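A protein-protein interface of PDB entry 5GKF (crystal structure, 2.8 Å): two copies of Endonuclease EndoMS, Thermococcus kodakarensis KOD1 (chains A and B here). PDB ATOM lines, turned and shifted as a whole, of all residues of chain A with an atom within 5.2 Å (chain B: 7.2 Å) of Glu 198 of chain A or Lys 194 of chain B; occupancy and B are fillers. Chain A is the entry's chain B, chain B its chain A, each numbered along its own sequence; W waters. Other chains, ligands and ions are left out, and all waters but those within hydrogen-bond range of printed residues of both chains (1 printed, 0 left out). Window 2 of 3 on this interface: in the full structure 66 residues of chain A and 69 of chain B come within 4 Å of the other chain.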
ATOM      1  N   LEU A 193      -9.671  30.905   5.261  1.00  0.00           N
ATOM      2  CA  LEU A 193      -8.522  31.063   6.134  1.00  0.00           C
ATOM      3  C   LEU A 193      -8.747  30.360   7.462  1.00  0.00           C
ATOM      4  O   LEU A 193      -7.859  29.694   7.964  1.00  0.00           O
ATOM      5  CB  LEU A 193      -8.227  32.535   6.375  1.00  0.00           C
ATOM      6  CG  LEU A 193      -7.153  32.884   7.419  1.00  0.00           C
ATOM      7  CD1 LEU A 193      -5.800  32.339   6.993  1.00  0.00           C
ATOM      8  CD2 LEU A 193      -7.090  34.403   7.702  1.00  0.00           C
ATOM      9  N   LYS A 194      -9.943  30.509   8.020  1.00  0.00           N
ATOM     10  CA  LYS A 194     -10.241  29.935   9.313  1.00  0.00           C
ATOM     11  C   LYS A 194     -10.184  28.431   9.248  1.00  0.00           C
ATOM     12  O   LYS A 194      -9.675  27.796  10.153  1.00  0.00           O
ATOM     13  CB  LYS A 194     -11.612  30.387   9.796  1.00  0.00           C
ATOM     14  CG  LYS A 194     -12.150  29.549  10.919  1.00  0.00           C
ATOM     15  CD  LYS A 194     -13.351  30.176  11.568  1.00  0.00           C
ATOM     16  CE  LYS A 194     -13.786  29.314  12.751  1.00  0.00           C
ATOM     17  NZ  LYS A 194     -14.655  28.180  12.370  1.00  0.00           N
ATOM     18  N   SER A 195     -10.690  27.876   8.152  1.00  0.00           N
ATOM     19  CA  SER A 195     -10.677  26.427   7.899  1.00  0.00           C
ATOM     20  C   SER A 195      -9.279  25.832   7.859  1.00  0.00           C
ATOM     21  O   SER A 195      -9.011  24.819   8.494  1.00  0.00           O
ATOM     22  CB  SER A 195     -11.378  26.116   6.576  1.00  0.00           C
ATOM     23  OG  SER A 195     -11.886  24.792   6.561  1.00  0.00           O
ATOM     24  N   TYR A 196      -8.411  26.459   7.076  1.00  0.00           N
ATOM     25  CA  TYR A 196      -6.999  26.114   6.988  1.00  0.00           C
ATOM     26  C   TYR A 196      -6.282  26.138   8.356  1.00  0.00           C
ATOM     27  O   TYR A 196      -5.416  25.307   8.651  1.00  0.00           O
ATOM     28  CB  TYR A 196      -6.300  27.084   6.042  1.00  0.00           C
ATOM     29  CG  TYR A 196      -6.895  27.158   4.654  1.00  0.00           C
ATOM     30  CD1 TYR A 196      -7.509  26.065   4.073  1.00  0.00           C
ATOM     31  CD2 TYR A 196      -6.818  28.321   3.918  1.00  0.00           C
ATOM     32  CE1 TYR A 196      -8.045  26.141   2.789  1.00  0.00           C
ATOM     33  CE2 TYR A 196      -7.337  28.401   2.659  1.00  0.00           C
ATOM     34  CZ  TYR A 196      -7.947  27.314   2.092  1.00  0.00           C
ATOM     35  OH  TYR A 196      -8.444  27.441   0.823  1.00  0.00           O
ATOM     36  N   VAL A 197      -6.653  27.098   9.187  1.00  0.00           N
ATOM     37  CA  VAL A 197      -5.943  27.353  10.420  1.00  0.00           C
ATOM     38  C   VAL A 197      -6.353  26.342  11.485  1.00  0.00           C
ATOM     39  O   VAL A 197      -5.504  25.832  12.208  1.00  0.00           O
ATOM     40  CB  VAL A 197      -6.195  28.789  10.890  1.00  0.00           C
ATOM     41  CG1 VAL A 197      -5.895  28.948  12.366  1.00  0.00           C
ATOM     42  CG2 VAL A 197      -5.384  29.762  10.043  1.00  0.00           C
ATOM     43  N   GLU A 198      -7.649  26.038  11.554  1.00  0.00           N
ATOM     44  CA  GLU A 198      -8.162  24.983  12.435  1.00  0.00           C
ATOM     45  C   GLU A 198      -7.485  23.668  12.128  1.00  0.00           C
ATOM     46  O   GLU A 198      -7.128  22.928  13.035  1.00  0.00           O
ATOM     47  CB  GLU A 198      -9.687  24.792  12.303  1.00  0.00           C
ATOM     48  CG  GLU A 198     -10.519  25.939  12.826  1.00  0.00           C
ATOM     49  CD  GLU A 198     -11.976  25.574  13.004  1.00  0.00           C
ATOM     50  OE1 GLU A 198     -12.300  24.365  12.994  1.00  0.00           O
ATOM     51  OE2 GLU A 198     -12.804  26.499  13.165  1.00  0.00           O
ATOM     52  N   ILE A 199      -7.322  23.390  10.839  1.00  0.00           N
ATOM     53  CA  ILE A 199      -6.696  22.158  10.391  1.00  0.00           C
ATOM     54  C   ILE A 199      -5.223  22.069  10.787  1.00  0.00           C
ATOM     55  O   ILE A 199      -4.763  21.033  11.251  1.00  0.00           O
ATOM     56  CB  ILE A 199      -6.828  22.014   8.876  1.00  0.00           C
ATOM     57  CG1 ILE A 199      -8.273  21.671   8.531  1.00  0.00           C
ATOM     58  CG2 ILE A 199      -5.852  20.953   8.343  1.00  0.00           C
ATOM     59  CD1 ILE A 199      -8.416  20.943   7.241  1.00  0.00           C
ATOM     60  N   LEU A 200      -4.487  23.159  10.625  1.00  0.00           N
ATOM     61  CA  LEU A 200      -3.084  23.120  10.967  1.00  0.00           C
ATOM     62  C   LEU A 200      -2.889  23.194  12.475  1.00  0.00           C
ATOM     63  O   LEU A 200      -1.885  22.694  12.972  1.00  0.00           O
ATOM     64  CB  LEU A 200      -2.319  24.234  10.266  1.00  0.00           C
ATOM     65  CG  LEU A 200      -2.185  24.052   8.744  1.00  0.00           C
ATOM     66  CD1 LEU A 200      -1.800  25.345   8.024  1.00  0.00           C
ATOM     67  CD2 LEU A 200      -1.190  22.971   8.407  1.00  0.00           C
ATOM     68  N   ARG A 201      -3.839  23.781  13.210  1.00  0.00           N
ATOM     69  CA  ARG A 201      -3.680  23.887  14.670  1.00  0.00           C
ATOM     70  C   ARG A 201      -3.677  22.491  15.242  1.00  0.00           C
ATOM     71  O   ARG A 201      -3.012  22.213  16.239  1.00  0.00           O
ATOM     72  CB  ARG A 201      -4.789  24.709  15.335  1.00  0.00           C
ATOM     73  CG  ARG A 201      -4.627  26.223  15.355  1.00  0.00           C
ATOM     74  CD  ARG A 201      -5.709  26.801  16.271  1.00  0.00           C
ATOM     75  NE  ARG A 201      -6.317  28.077  15.861  1.00  0.00           N
ATOM     76  CZ  ARG A 201      -5.649  29.223  15.788  1.00  0.00           C
ATOM     77  NH1 ARG A 201      -4.347  29.229  16.039  1.00  0.00           N
ATOM     78  NH2 ARG A 201      -6.267  30.349  15.439  1.00  0.00           N
ATOM     79  N   GLU A 202      -4.420  21.615  14.580  1.00  0.00           N
ATOM     80  CA  GLU A 202      -4.524  20.228  14.983  1.00  0.00           C
ATOM     81  C   GLU A 202      -3.171  19.511  14.951  1.00  0.00           C
ATOM     82  O   GLU A 202      -2.952  18.604  15.750  1.00  0.00           O
ATOM     83  CB  GLU A 202      -5.534  19.486  14.094  1.00  0.00           C
ATOM     84  CG  GLU A 202      -6.993  19.760  14.446  1.00  0.00           C
ATOM     85  CD  GLU A 202      -7.968  19.250  13.389  1.00  0.00           C
ATOM     86  OE1 GLU A 202      -7.532  18.451  12.523  1.00  0.00           O
ATOM     87  OE2 GLU A 202      -9.161  19.661  13.420  1.00  0.00           O
ATOM     88  N   GLU B 179     -27.795  23.620   4.253  1.00  0.00           N
ATOM     89  CA  GLU B 179     -27.074  24.256   3.154  1.00  0.00           C
ATOM     90  C   GLU B 179     -27.447  23.504   1.892  1.00  0.00           C
ATOM     91  O   GLU B 179     -27.277  22.285   1.829  1.00  0.00           O
ATOM     92  CB  GLU B 179     -25.557  24.256   3.372  1.00  0.00           C
ATOM     93  CG  GLU B 179     -24.744  25.040   2.302  1.00  0.00           C
ATOM     94  CD  GLU B 179     -25.209  26.486   2.096  1.00  0.00           C
ATOM     95  OE1 GLU B 179     -24.966  27.041   0.996  1.00  0.00           O
ATOM     96  OE2 GLU B 179     -25.813  27.076   3.032  1.00  0.00           O
ATOM     97  N   ALA B 189     -18.870  24.461   0.262  1.00  0.00           N
ATOM     98  CA  ALA B 189     -20.193  24.194   0.814  1.00  0.00           C
ATOM     99  C   ALA B 189     -20.163  23.746   2.291  1.00  0.00           C
ATOM    100  O   ALA B 189     -21.029  24.112   3.103  1.00  0.00           O
ATOM    101  CB  ALA B 189     -20.886  23.148  -0.024  1.00  0.00           C
ATOM    102  N   VAL B 190     -19.173  22.945   2.645  1.00  0.00           N
ATOM    103  CA  VAL B 190     -19.127  22.436   3.999  1.00  0.00           C
ATOM    104  C   VAL B 190     -18.604  23.521   4.939  1.00  0.00           C
ATOM    105  O   VAL B 190     -19.041  23.605   6.065  1.00  0.00           O
ATOM    106  CB  VAL B 190     -18.292  21.153   4.075  1.00  0.00           C
ATOM    107  CG1 VAL B 190     -18.207  20.672   5.495  1.00  0.00           C
ATOM    108  CG2 VAL B 190     -18.948  20.075   3.219  1.00  0.00           C
ATOM    109  N   ARG B 191     -17.707  24.376   4.455  1.00  0.00           N
ATOM    110  CA  ARG B 191     -17.245  25.534   5.216  1.00  0.00           C
ATOM    111  C   ARG B 191     -18.392  26.494   5.508  1.00  0.00           C
ATOM    112  O   ARG B 191     -18.489  27.038   6.592  1.00  0.00           O
ATOM    113  CB  ARG B 191     -16.138  26.293   4.469  1.00  0.00           C
ATOM    114  CG  ARG B 191     -14.929  25.482   4.134  1.00  0.00           C
ATOM    115  CD  ARG B 191     -13.726  26.335   4.003  1.00  0.00           C
ATOM    116  NE  ARG B 191     -12.632  25.598   3.384  1.00  0.00           N
ATOM    117  CZ  ARG B 191     -12.379  25.584   2.077  1.00  0.00           C
ATOM    118  NH1 ARG B 191     -13.129  26.291   1.222  1.00  0.00           N
ATOM    119  NH2 ARG B 191     -11.365  24.862   1.629  1.00  0.00           N
ATOM    120  N   GLN B 192     -19.239  26.731   4.518  1.00  0.00           N
ATOM    121  CA  GLN B 192     -20.431  27.518   4.729  1.00  0.00           C
ATOM    122  C   GLN B 192     -21.234  26.878   5.872  1.00  0.00           C
ATOM    123  O   GLN B 192     -21.503  27.525   6.882  1.00  0.00           O
ATOM    124  CB  GLN B 192     -21.271  27.595   3.445  1.00  0.00           C
ATOM    125  CG  GLN B 192     -21.135  28.860   2.612  1.00  0.00           C
ATOM    126  CD  GLN B 192     -22.131  28.904   1.428  1.00  0.00           C
ATOM    127  OE1 GLN B 192     -23.353  29.165   1.583  1.00  0.00           O
ATOM    128  NE2 GLN B 192     -21.604  28.656   0.244  1.00  0.00           N
ATOM    129  N   LEU B 193     -21.580  25.599   5.716  1.00  0.00           N
ATOM    130  CA  LEU B 193     -22.431  24.907   6.682  1.00  0.00           C
ATOM    131  C   LEU B 193     -21.809  24.968   8.080  1.00  0.00           C
ATOM    132  O   LEU B 193     -22.419  25.481   9.015  1.00  0.00           O
ATOM    133  CB  LEU B 193     -22.657  23.453   6.256  1.00  0.00           C
ATOM    134  CG  LEU B 193     -23.557  22.524   7.071  1.00  0.00           C
ATOM    135  CD1 LEU B 193     -24.936  23.113   7.286  1.00  0.00           C
ATOM    136  CD2 LEU B 193     -23.680  21.182   6.392  1.00  0.00           C
ATOM    137  N   LYS B 194     -20.578  24.477   8.199  1.00  0.00           N
ATOM    138  CA  LYS B 194     -19.837  24.504   9.447  1.00  0.00           C
ATOM    139  C   LYS B 194     -19.787  25.895  10.101  1.00  0.00           C
ATOM    140  O   LYS B 194     -19.782  26.025  11.323  1.00  0.00           O
ATOM    141  CB  LYS B 194     -18.430  24.011   9.214  1.00  0.00           C
ATOM    142  CG  LYS B 194     -17.674  23.773  10.479  1.00  0.00           C
ATOM    143  CD  LYS B 194     -16.212  24.099  10.325  1.00  0.00           C
ATOM    144  CE  LYS B 194     -15.488  23.683  11.576  1.00  0.00           C
ATOM    145  NZ  LYS B 194     -14.305  24.511  11.872  1.00  0.00           N
ATOM    146  N   SER B 195     -19.757  26.943   9.295  1.00  0.00           N
ATOM    147  CA  SER B 195     -19.742  28.278   9.859  1.00  0.00           C
ATOM    148  C   SER B 195     -21.088  28.581  10.502  1.00  0.00           C
ATOM    149  O   SER B 195     -21.154  29.058  11.628  1.00  0.00           O
ATOM    150  CB  SER B 195     -19.411  29.305   8.788  1.00  0.00           C
ATOM    151  OG  SER B 195     -19.516  30.626   9.277  1.00  0.00           O
ATOM    152  N   TYR B 196     -22.160  28.284   9.784  1.00  0.00           N
ATOM    153  CA  TYR B 196     -23.504  28.600  10.252  1.00  0.00           C
ATOM    154  C   TYR B 196     -23.820  27.835  11.525  1.00  0.00           C
ATOM    155  O   TYR B 196     -24.407  28.377  12.470  1.00  0.00           O
ATOM    156  CB  TYR B 196     -24.547  28.277   9.177  1.00  0.00           C
ATOM    157  CG  TYR B 196     -24.323  29.025   7.880  1.00  0.00           C
ATOM    158  CD1 TYR B 196     -23.807  30.312   7.875  1.00  0.00           C
ATOM    159  CD2 TYR B 196     -24.612  28.431   6.656  1.00  0.00           C
ATOM    160  CE1 TYR B 196     -23.599  30.988   6.685  1.00  0.00           C
ATOM    161  CE2 TYR B 196     -24.402  29.090   5.474  1.00  0.00           C
ATOM    162  CZ  TYR B 196     -23.891  30.367   5.486  1.00  0.00           C
ATOM    163  OH  TYR B 196     -23.692  31.025   4.285  1.00  0.00           O
ATOM    164  N   VAL B 197     -23.418  26.571  11.536  1.00  0.00           N
ATOM    165  CA  VAL B 197     -23.722  25.690  12.637  1.00  0.00           C
ATOM    166  C   VAL B 197     -22.997  26.184  13.872  1.00  0.00           C
ATOM    167  O   VAL B 197     -23.514  26.102  14.981  1.00  0.00           O
ATOM    168  CB  VAL B 197     -23.342  24.243  12.303  1.00  0.00           C
ATOM    169  CG1 VAL B 197     -23.232  23.379  13.569  1.00  0.00           C
ATOM    170  CG2 VAL B 197     -24.367  23.667  11.339  1.00  0.00           C
ATOM    171  N   GLU B 198     -21.815  26.747  13.669  1.00  0.00           N
ATOM    172  CA  GLU B 198     -21.023  27.245  14.780  1.00  0.00           C
ATOM    173  C   GLU B 198     -21.678  28.464  15.394  1.00  0.00           C
ATOM    174  O   GLU B 198     -21.936  28.511  16.600  1.00  0.00           O
ATOM    175  CB  GLU B 198     -19.594  27.552  14.324  1.00  0.00           C
ATOM    176  CG  GLU B 198     -18.685  26.366  14.593  1.00  0.00           C
ATOM    177  CD  GLU B 198     -17.332  26.474  13.956  1.00  0.00           C
ATOM    178  OE1 GLU B 198     -16.888  27.610  13.666  1.00  0.00           O
ATOM    179  OE2 GLU B 198     -16.725  25.401  13.739  1.00  0.00           O
ATOM    180  N   ILE B 199     -21.973  29.433  14.542  1.00  0.00           N
ATOM    181  CA  ILE B 199     -22.564  30.687  14.972  1.00  0.00           C
ATOM    182  C   ILE B 199     -23.921  30.491  15.682  1.00  0.00           C
ATOM    183  O   ILE B 199     -24.239  31.212  16.621  1.00  0.00           O
ATOM    184  CB  ILE B 199     -22.681  31.616  13.757  1.00  0.00           C
ATOM    185  CG1 ILE B 199     -21.283  32.110  13.381  1.00  0.00           C
ATOM    186  CG2 ILE B 199     -23.674  32.753  14.001  1.00  0.00           C
ATOM    187  CD1 ILE B 199     -21.271  33.185  12.336  1.00  0.00           C
ATOM    188  N   LEU B 200     -24.685  29.487  15.260  1.00  0.00           N
ATOM    189  CA  LEU B 200     -25.939  29.123  15.920  1.00  0.00           C
ATOM    190  C   LEU B 200     -25.751  28.329  17.219  1.00  0.00           C
ATOM    191  O   LEU B 200     -26.570  28.479  18.118  1.00  0.00           O
ATOM    192  CB  LEU B 200     -26.828  28.327  14.958  1.00  0.00           C
ATOM    193  CG  LEU B 200     -27.581  29.279  14.033  1.00  0.00           C
ATOM    194  CD1 LEU B 200     -28.073  28.579  12.816  1.00  0.00           C
ATOM    195  CD2 LEU B 200     -28.733  29.901  14.777  1.00  0.00           C
ATOM    196  N   ARG B 201     -24.705  27.494  17.326  1.00  0.00           N
ATOM    197  CA  ARG B 201     -24.397  26.799  18.595  1.00  0.00           C
ATOM    198  C   ARG B 201     -24.029  27.818  19.697  1.00  0.00           C
ATOM    199  O   ARG B 201     -24.284  27.599  20.890  1.00  0.00           O
ATOM    200  CB  ARG B 201     -23.256  25.777  18.439  1.00  0.00           C
ATOM    201  CG  ARG B 201     -23.616  24.439  17.778  1.00  0.00           C
ATOM    202  CD  ARG B 201     -22.512  23.376  18.011  1.00  0.00           C
ATOM    203  NE  ARG B 201     -22.399  22.399  16.921  1.00  0.00           N
ATOM    204  CZ  ARG B 201     -23.212  21.355  16.732  1.00  0.00           C
ATOM    205  NH1 ARG B 201     -24.226  21.144  17.565  1.00  0.00           N
ATOM    206  NH2 ARG B 201     -23.021  20.522  15.701  1.00  0.00           N
ATOM    207  N   GLY B 210     -26.271  20.619  11.481  1.00  0.00           N
ATOM    208  CA  GLY B 210     -26.139  20.986  10.081  1.00  0.00           C
ATOM    209  C   GLY B 210     -26.455  19.860   9.105  1.00  0.00           C
ATOM    210  O   GLY B 210     -25.974  18.742   9.246  1.00  0.00           O
ATOM    211  N   LEU B 224     -14.316  16.234   5.094  1.00  0.00           N
ATOM    212  CA  LEU B 224     -14.597  17.303   6.051  1.00  0.00           C
ATOM    213  C   LEU B 224     -15.998  17.237   6.678  1.00  0.00           C
ATOM    214  O   LEU B 224     -16.194  17.650   7.818  1.00  0.00           O
ATOM    215  CB  LEU B 224     -14.408  18.665   5.379  1.00  0.00           C
ATOM    216  CG  LEU B 224     -14.568  19.890   6.294  1.00  0.00           C
ATOM    217  CD1 LEU B 224     -13.499  19.879   7.347  1.00  0.00           C
ATOM    218  CD2 LEU B 224     -14.553  21.228   5.540  1.00  0.00           C
ATOM    219  N   LEU B 225     -16.974  16.738   5.939  1.00  0.00           N
ATOM    220  CA  LEU B 225     -18.330  16.680   6.473  1.00  0.00           C
ATOM    221  C   LEU B 225     -18.333  15.762   7.673  1.00  0.00           C
ATOM    222  O   LEU B 225     -18.721  16.156   8.764  1.00  0.00           O
ATOM    223  CB  LEU B 225     -19.344  16.185   5.432  1.00  0.00           C
ATOM    224  CG  LEU B 225     -20.799  16.410   5.849  1.00  0.00           C
ATOM    225  CD1 LEU B 225     -21.200  17.882   5.698  1.00  0.00           C
ATOM    226  CD2 LEU B 225     -21.757  15.498   5.106  1.00  0.00           C
ATOM    227  N   LYS B 227     -15.781  14.599   9.457  1.00  0.00           N
ATOM    228  CA  LYS B 227     -14.900  15.048  10.524  1.00  0.00           C
ATOM    229  C   LYS B 227     -15.620  15.971  11.517  1.00  0.00           C
ATOM    230  O   LYS B 227     -15.700  15.646  12.700  1.00  0.00           O
ATOM    231  CB  LYS B 227     -13.671  15.733   9.920  1.00  0.00           C
ATOM    232  CG  LYS B 227     -12.766  16.461  10.903  1.00  0.00           C
ATOM    233  CD  LYS B 227     -11.485  16.982  10.219  1.00  0.00           C
ATOM    234  CE  LYS B 227     -10.669  17.908  11.133  1.00  0.00           C
ATOM    235  NZ  LYS B 227     -11.181  19.318  11.224  1.00  0.00           N
ATOM    236  N   GLU B 228     -16.213  17.071  11.054  1.00  0.00           N
ATOM    237  CA  GLU B 228     -16.854  18.019  11.985  1.00  0.00           C
ATOM    238  C   GLU B 228     -18.264  17.545  12.322  1.00  0.00           C
ATOM    239  O   GLU B 228     -19.068  18.284  12.892  1.00  0.00           O
ATOM    240  CB  GLU B 228     -16.865  19.462  11.450  1.00  0.00           C
ATOM    241  CG  GLU B 228     -16.039  20.450  12.334  1.00  0.00           C
ATOM    242  CD  GLU B 228     -16.669  20.801  13.728  1.00  0.00           C
ATOM    243  OE1 GLU B 228     -17.716  21.502  13.782  1.00  0.00           O
ATOM    244  OE2 GLU B 228     -16.091  20.411  14.780  1.00  0.00           O
ATOM    245  N   LEU B 230     -21.102  16.665  10.485  1.00  0.00           N
ATOM    246  CA  LEU B 230     -22.336  17.206   9.922  1.00  0.00           C
ATOM    247  C   LEU B 230     -22.986  16.103   9.099  1.00  0.00           C
ATOM    248  O   LEU B 230     -22.396  15.028   8.960  1.00  0.00           O
ATOM    249  CB  LEU B 230     -22.051  18.459   9.093  1.00  0.00           C
ATOM    250  CG  LEU B 230     -21.303  19.568   9.840  1.00  0.00           C
ATOM    251  CD1 LEU B 230     -21.000  20.746   8.948  1.00  0.00           C
ATOM    252  CD2 LEU B 230     -22.116  20.039  11.018  1.00  0.00           C
HETATM  253  O   HOH W   1     -13.791  22.084  15.096  1.00  0.00           O
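Of the printed residues of chain B, Glu 198 of chain A touches Lys 194.
Printed residues of chain A within 4 Å of Arg 191 of chain B: Ser 195 and Tyr 196.
Of the printed residues of chain B, Ser 195 of chain A touches Arg 191.
Arg 201 of chain B touches none of the printed residues of chain A.
Val 190 of chain B touches none of the printed residues of chain A.
The nearest printed residue of chain A that does not touch Lys 194 of chain B is Ser 195 of chain A (5.7 Å).
The nearest printed residue of chain B that does not touch Glu 202 of chain A is Glu 228 of chain B (7.0 Å).
The side-chain amino group of Lys 194 of chain B lies within salt-bridge range of the side-chain carboxylate of Glu 198 of chain B, 3.2 Å away.
OE2 of Glu 198 of chain A is in salt-bridge range of NZ of Lys 194 of chain A (2.6 Å).
Among the printed residues, merely in contact across the chains: Lys 194 of chain A with Lys 194 of chain B and Tyr 196 of chain A with Arg 191 of chain B.
Lys 194 of chain A touches its own counterpart, Lys 194 of chain B.
Lys 194 of chain A touches Glu 198 of chain B, and with the chains exchanged Glu 198 of chain A touches Lys 194 of chain B.
Water W1 lies within hydrogen-bond range of the side-chain carboxylate (OE2) of Glu 228 of chain B (2.9 Å) and the side-chain carboxylate (OE1) of Glu 198 of chain A (3.4 Å).
Printed residues of chain B that touch a printed residue of chain A: Arg 191, Lys 194, Glu 198 and Lys 227.
Along chain B the printed residues that touch a printed residue of chain A span positions 191 to 227.
Among the printed residues, Asp or Glu carboxylates within 4 Å of a Lys or Arg side-chain nitrogen of the other chain: Lys 194 of chain A with Glu 198 of chain B, Glu 198 of chain A with Lys 194 of chain B and Glu 202 of chain A with Lys 227 of chain B.
NZ of Lys 194 of chain A is in salt-bridge range of OE1 of Glu 198 of chain B (2.6 Å).
OE2 of Glu 198 of chain A lies within salt-bridge range of NZ of Lys 194 of chain B (2.8 Å).
NZ of Lys 227 of chain B lies within salt-bridge range of OE2 of Glu 202 of chain A (3.0 Å).
NE of Arg 191 of chain B lies within hydrogen-bond range of OG of Ser 195 of chain A (3.4 Å).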
